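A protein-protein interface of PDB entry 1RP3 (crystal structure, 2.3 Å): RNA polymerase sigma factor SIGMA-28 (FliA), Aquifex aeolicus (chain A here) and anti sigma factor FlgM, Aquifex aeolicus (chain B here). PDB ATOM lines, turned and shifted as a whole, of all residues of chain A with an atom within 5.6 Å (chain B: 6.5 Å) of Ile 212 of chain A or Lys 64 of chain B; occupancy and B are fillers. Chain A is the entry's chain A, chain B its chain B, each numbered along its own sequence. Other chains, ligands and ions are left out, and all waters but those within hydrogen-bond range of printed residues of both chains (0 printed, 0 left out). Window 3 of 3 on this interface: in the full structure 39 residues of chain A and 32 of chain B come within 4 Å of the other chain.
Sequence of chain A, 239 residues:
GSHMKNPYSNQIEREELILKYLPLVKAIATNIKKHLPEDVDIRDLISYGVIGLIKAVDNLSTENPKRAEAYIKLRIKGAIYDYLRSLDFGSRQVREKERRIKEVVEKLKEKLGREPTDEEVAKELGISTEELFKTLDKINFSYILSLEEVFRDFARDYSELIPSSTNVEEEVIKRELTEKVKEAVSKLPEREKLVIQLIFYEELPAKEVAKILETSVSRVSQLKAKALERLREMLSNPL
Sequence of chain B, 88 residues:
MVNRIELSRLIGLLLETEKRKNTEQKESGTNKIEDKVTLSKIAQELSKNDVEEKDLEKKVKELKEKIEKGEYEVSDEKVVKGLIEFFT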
ATOM      1  N   LEU A 198      -4.463 -15.521  18.355  1.00  0.00           N
ATOM      2  CA  LEU A 198      -3.491 -14.443  18.513  1.00  0.00           C
ATOM      3  C   LEU A 198      -2.819 -14.088  17.192  1.00  0.00           C
ATOM      4  O   LEU A 198      -2.487 -12.924  16.942  1.00  0.00           O
ATOM      5  CB  LEU A 198      -2.433 -14.805  19.557  1.00  0.00           C
ATOM      6  CG  LEU A 198      -2.816 -14.809  21.045  1.00  0.00           C
ATOM      7  CD1 LEU A 198      -1.607 -15.190  21.867  1.00  0.00           C
ATOM      8  CD2 LEU A 198      -3.331 -13.463  21.496  1.00  0.00           C
ATOM      9  N   LEU A 204      -0.992 -10.941  14.866  1.00  0.00           N
ATOM     10  CA  LEU A 204       0.326 -10.843  15.456  1.00  0.00           C
ATOM     11  C   LEU A 204       1.268 -11.893  14.914  1.00  0.00           C
ATOM     12  O   LEU A 204       0.915 -13.055  14.838  1.00  0.00           O
ATOM     13  CB  LEU A 204       0.223 -11.002  16.971  1.00  0.00           C
ATOM     14  CG  LEU A 204      -0.526  -9.887  17.697  1.00  0.00           C
ATOM     15  CD1 LEU A 204      -0.556 -10.197  19.178  1.00  0.00           C
ATOM     16  CD2 LEU A 204       0.136  -8.538  17.430  1.00  0.00           C
ATOM     17  N   GLU A 208       5.781 -12.156  18.183  1.00  0.00           N
ATOM     18  CA  GLU A 208       5.029 -11.433  19.198  1.00  0.00           C
ATOM     19  C   GLU A 208       4.215 -12.398  20.037  1.00  0.00           C
ATOM     20  O   GLU A 208       4.037 -12.201  21.239  1.00  0.00           O
ATOM     21  CB  GLU A 208       4.101 -10.410  18.553  1.00  0.00           C
ATOM     22  CG  GLU A 208       4.811  -9.428  17.641  1.00  0.00           C
ATOM     23  CD  GLU A 208       5.983  -8.717  18.316  1.00  0.00           C
ATOM     24  OE1 GLU A 208       5.862  -8.322  19.494  1.00  0.00           O
ATOM     25  OE2 GLU A 208       7.034  -8.544  17.661  1.00  0.00           O
ATOM     26  N   VAL A 209       3.724 -13.453  19.404  1.00  0.00           N
ATOM     27  CA  VAL A 209       2.928 -14.437  20.111  1.00  0.00           C
ATOM     28  C   VAL A 209       3.809 -15.146  21.133  1.00  0.00           C
ATOM     29  O   VAL A 209       3.361 -15.457  22.234  1.00  0.00           O
ATOM     30  CB  VAL A 209       2.291 -15.423  19.130  1.00  0.00           C
ATOM     31  CG1 VAL A 209       1.599 -16.538  19.876  1.00  0.00           C
ATOM     32  CG2 VAL A 209       1.286 -14.682  18.246  1.00  0.00           C
ATOM     33  N   ALA A 210       5.081 -15.331  20.787  1.00  0.00           N
ATOM     34  CA  ALA A 210       6.042 -15.980  21.677  1.00  0.00           C
ATOM     35  C   ALA A 210       6.239 -15.193  22.978  1.00  0.00           C
ATOM     36  O   ALA A 210       6.375 -15.774  24.050  1.00  0.00           O
ATOM     37  CB  ALA A 210       7.384 -16.165  20.964  1.00  0.00           C
ATOM     38  N   LYS A 211       6.249 -13.868  22.866  1.00  0.00           N
ATOM     39  CA  LYS A 211       6.420 -12.988  24.015  1.00  0.00           C
ATOM     40  C   LYS A 211       5.188 -13.032  24.918  1.00  0.00           C
ATOM     41  O   LYS A 211       5.303 -13.081  26.144  1.00  0.00           O
ATOM     42  CB  LYS A 211       6.699 -11.557  23.541  1.00  0.00           C
ATOM     43  CG  LYS A 211       8.011 -11.424  22.766  1.00  0.00           C
ATOM     44  CD  LYS A 211       8.066 -10.194  21.857  1.00  0.00           C
ATOM     45  CE  LYS A 211       8.064  -8.876  22.623  1.00  0.00           C
ATOM     46  NZ  LYS A 211       8.179  -7.722  21.678  1.00  0.00           N
ATOM     47  N   ILE A 212       4.011 -13.062  24.300  1.00  0.00           N
ATOM     48  CA  ILE A 212       2.757 -13.110  25.039  1.00  0.00           C
ATOM     49  C   ILE A 212       2.643 -14.418  25.815  1.00  0.00           C
ATOM     50  O   ILE A 212       2.377 -14.403  27.014  1.00  0.00           O
ATOM     51  CB  ILE A 212       1.531 -12.949  24.090  1.00  0.00           C
ATOM     52  CG1 ILE A 212       1.612 -11.619  23.347  1.00  0.00           C
ATOM     53  CG2 ILE A 212       0.242 -12.976  24.870  1.00  0.00           C
ATOM     54  CD1 ILE A 212       0.566 -11.461  22.282  1.00  0.00           C
ATOM     55  N   LEU A 213       2.858 -15.547  25.143  1.00  0.00           N
ATOM     56  CA  LEU A 213       2.748 -16.849  25.804  1.00  0.00           C
ATOM     57  C   LEU A 213       3.968 -17.266  26.639  1.00  0.00           C
ATOM     58  O   LEU A 213       3.982 -18.349  27.247  1.00  0.00           O
ATOM     59  CB  LEU A 213       2.370 -17.937  24.795  1.00  0.00           C
ATOM     60  CG  LEU A 213       1.047 -17.676  24.063  1.00  0.00           C
ATOM     61  CD1 LEU A 213       0.689 -18.867  23.182  1.00  0.00           C
ATOM     62  CD2 LEU A 213      -0.068 -17.402  25.070  1.00  0.00           C
ATOM     63  N   GLU A 214       4.965 -16.383  26.696  1.00  0.00           N
ATOM     64  CA  GLU A 214       6.192 -16.611  27.454  1.00  0.00           C
ATOM     65  C   GLU A 214       6.927 -17.895  27.061  1.00  0.00           C
ATOM     66  O   GLU A 214       7.473 -18.591  27.918  1.00  0.00           O
ATOM     67  CB  GLU A 214       5.897 -16.599  28.953  1.00  0.00           C
ATOM     68  N   LYS B  59      -0.030  -3.306  22.420  1.00  0.00           N
ATOM     69  CA  LYS B  59      -0.996  -4.367  22.144  1.00  0.00           C
ATOM     70  C   LYS B  59      -0.515  -5.683  22.736  1.00  0.00           C
ATOM     71  O   LYS B  59      -1.304  -6.445  23.297  1.00  0.00           O
ATOM     72  CB  LYS B  59      -1.190  -4.523  20.635  1.00  0.00           C
ATOM     73  CG  LYS B  59      -2.241  -5.546  20.241  1.00  0.00           C
ATOM     74  CD  LYS B  59      -2.438  -5.570  18.740  1.00  0.00           C
ATOM     75  CE  LYS B  59      -3.600  -6.466  18.354  1.00  0.00           C
ATOM     76  NZ  LYS B  59      -3.895  -6.373  16.900  1.00  0.00           N
ATOM     77  N   VAL B  60       0.787  -5.935  22.606  1.00  0.00           N
ATOM     78  CA  VAL B  60       1.408  -7.146  23.122  1.00  0.00           C
ATOM     79  C   VAL B  60       1.284  -7.168  24.639  1.00  0.00           C
ATOM     80  O   VAL B  60       0.802  -8.144  25.215  1.00  0.00           O
ATOM     81  CB  VAL B  60       2.901  -7.224  22.723  1.00  0.00           C
ATOM     82  CG1 VAL B  60       3.574  -8.403  23.408  1.00  0.00           C
ATOM     83  CG2 VAL B  60       3.033  -7.363  21.219  1.00  0.00           C
ATOM     84  N   LYS B  61       1.687  -6.070  25.274  1.00  0.00           N
ATOM     85  CA  LYS B  61       1.622  -5.950  26.726  1.00  0.00           C
ATOM     86  C   LYS B  61       0.186  -6.083  27.235  1.00  0.00           C
ATOM     87  O   LYS B  61      -0.088  -6.886  28.129  1.00  0.00           O
ATOM     88  CB  LYS B  61       2.222  -4.627  27.169  1.00  0.00           C
ATOM     89  N   GLU B  62      -0.726  -5.315  26.642  1.00  0.00           N
ATOM     90  CA  GLU B  62      -2.134  -5.340  27.028  1.00  0.00           C
ATOM     91  C   GLU B  62      -2.718  -6.743  26.889  1.00  0.00           C
ATOM     92  O   GLU B  62      -3.490  -7.191  27.739  1.00  0.00           O
ATOM     93  CB  GLU B  62      -2.931  -4.349  26.188  1.00  0.00           C
ATOM     94  N   LEU B  63      -2.324  -7.438  25.824  1.00  0.00           N
ATOM     95  CA  LEU B  63      -2.795  -8.796  25.563  1.00  0.00           C
ATOM     96  C   LEU B  63      -2.204  -9.804  26.546  1.00  0.00           C
ATOM     97  O   LEU B  63      -2.925 -10.641  27.083  1.00  0.00           O
ATOM     98  CB  LEU B  63      -2.463  -9.211  24.125  1.00  0.00           C
ATOM     99  CG  LEU B  63      -3.629  -9.413  23.153  1.00  0.00           C
ATOM    100  CD1 LEU B  63      -4.505  -8.171  23.090  1.00  0.00           C
ATOM    101  CD2 LEU B  63      -3.079  -9.738  21.784  1.00  0.00           C
ATOM    102  N   LYS B  64      -0.894  -9.713  26.781  1.00  0.00           N
ATOM    103  CA  LYS B  64      -0.198 -10.616  27.703  1.00  0.00           C
ATOM    104  C   LYS B  64      -0.700 -10.434  29.132  1.00  0.00           C
ATOM    105  O   LYS B  64      -0.957 -11.411  29.839  1.00  0.00           O
ATOM    106  CB  LYS B  64       1.313 -10.386  27.638  1.00  0.00           C
ATOM    107  N   GLU B  65      -0.847  -9.173  29.538  1.00  0.00           N
ATOM    108  CA  GLU B  65      -1.339  -8.827  30.869  1.00  0.00           C
ATOM    109  C   GLU B  65      -2.760  -9.354  31.053  1.00  0.00           C
ATOM    110  O   GLU B  65      -3.127  -9.798  32.139  1.00  0.00           O
ATOM    111  CB  GLU B  65      -1.309  -7.312  31.068  1.00  0.00           C
ATOM    112  N   LYS B  66      -3.546  -9.319  29.978  1.00  0.00           N
ATOM    113  CA  LYS B  66      -4.924  -9.796  30.005  1.00  0.00           C
ATOM    114  C   LYS B  66      -5.008 -11.322  29.992  1.00  0.00           C
ATOM    115  O   LYS B  66      -5.976 -11.892  30.482  1.00  0.00           O
ATOM    116  CB  LYS B  66      -5.709  -9.213  28.837  1.00  0.00           C
ATOM    117  N   ILE B  67      -4.000 -11.982  29.422  1.00  0.00           N
ATOM    118  CA  ILE B  67      -3.984 -13.445  29.364  1.00  0.00           C
ATOM    119  C   ILE B  67      -3.547 -14.031  30.701  1.00  0.00           C
ATOM    120  O   ILE B  67      -4.003 -15.107  31.099  1.00  0.00           O
ATOM    121  CB  ILE B  67      -3.060 -13.968  28.240  1.00  0.00           C
ATOM    122  CG1 ILE B  67      -3.588 -13.505  26.882  1.00  0.00           C
ATOM    123  CG2 ILE B  67      -2.997 -15.492  28.265  1.00  0.00           C
ATOM    124  CD1 ILE B  67      -2.766 -13.959  25.708  1.00  0.00           C
ATOM    125  N   GLU B  68      -2.652 -13.320  31.383  1.00  0.00           N
ATOM    126  CA  GLU B  68      -2.157 -13.750  32.684  1.00  0.00           C
ATOM    127  C   GLU B  68      -3.216 -13.461  33.736  1.00  0.00           C
ATOM    128  O   GLU B  68      -3.386 -14.229  34.685  1.00  0.00           O
ATOM    129  CB  GLU B  68      -0.861 -13.021  33.028  1.00  0.00           C
ATOM    130  CG  GLU B  68       0.254 -13.298  32.041  1.00  0.00           C
ATOM    131  CD  GLU B  68       1.494 -12.463  32.290  1.00  0.00           C
ATOM    132  OE1 GLU B  68       1.372 -11.338  32.833  1.00  0.00           O
ATOM    133  OE2 GLU B  68       2.592 -12.934  31.922  1.00  0.00           O
ATOM    134  N   LYS B  69      -3.931 -12.351  33.554  1.00  0.00           N
ATOM    135  CA  LYS B  69      -4.999 -11.955  34.469  1.00  0.00           C
ATOM    136  C   LYS B  69      -6.229 -12.839  34.245  1.00  0.00           C
ATOM    137  O   LYS B  69      -7.241 -12.696  34.937  1.00  0.00           O
ATOM    138  CB  LYS B  69      -5.358 -10.476  34.265  1.00  0.00           C
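Leu 63 of chain B touches Leu 198 of chain A (CD2 to CD2, 3.7 Å).
Leu 204 of chain A touches Leu 63 of chain B (CD1 to CD2, 3.7 Å).
Val 60 of chain B touches Glu 208 of chain A (CG2 to OE1, 3.4 Å).
Val 60 of chain B touches Ile 212 of chain A (CG1 to CG1, 3.8 Å).
Ile 212 of chain A touches Lys 64 of chain B.
Ile 212 of chain A touches Ile 67 of chain B.
Lys 64 of chain B touches just one residue of chain A: Ile 212 (3.7 Å).
Of the printed residues of chain B, Leu 204 of chain A touches Leu 63 (3.7 Å).
Printed residues of chain A within 4 Å of Leu 63 of chain B: Leu 198 and Leu 204.
Printed residues of chain A within 4 Å of Val 60 of chain B: Glu 208 and Ile 212.
Printed residues of chain A within 4 Å of Ile 67 of chain B: Ile 212.
Lys 61 of chain B touches none of the printed residues of chain A.
Lys 211 of chain A touches none of the printed residues of chain B.
The nearest residue of chain B that does not touch Ile 212 of chain A is Leu 63 of chain B (4.1 Å).
Of the 9 printed residues of chain A, 4 touch a printed residue of chain B.
Printed residues of chain A that touch a printed residue of chain B: Leu 198, Leu 204, Glu 208 and Ile 212.
Hydrophobic or aromatic side chains of chain A that line the printed part of chain B: Leu 198, Leu 204 and Ile 212.
Printed residues of chain B that touch a printed residue of chain A: Val 60, Leu 63, Lys 64 and Ile 67.
Along chain B the printed residues that touch a printed residue of chain A span positions 60 to 67.
N of Leu 204 of chain A is in hydrogen-bond range of O of Leu 198 of chain A.
OE1 of Glu 208 of chain A is in salt-bridge range of NZ of Lys 211 of chain A (3.2 Å).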
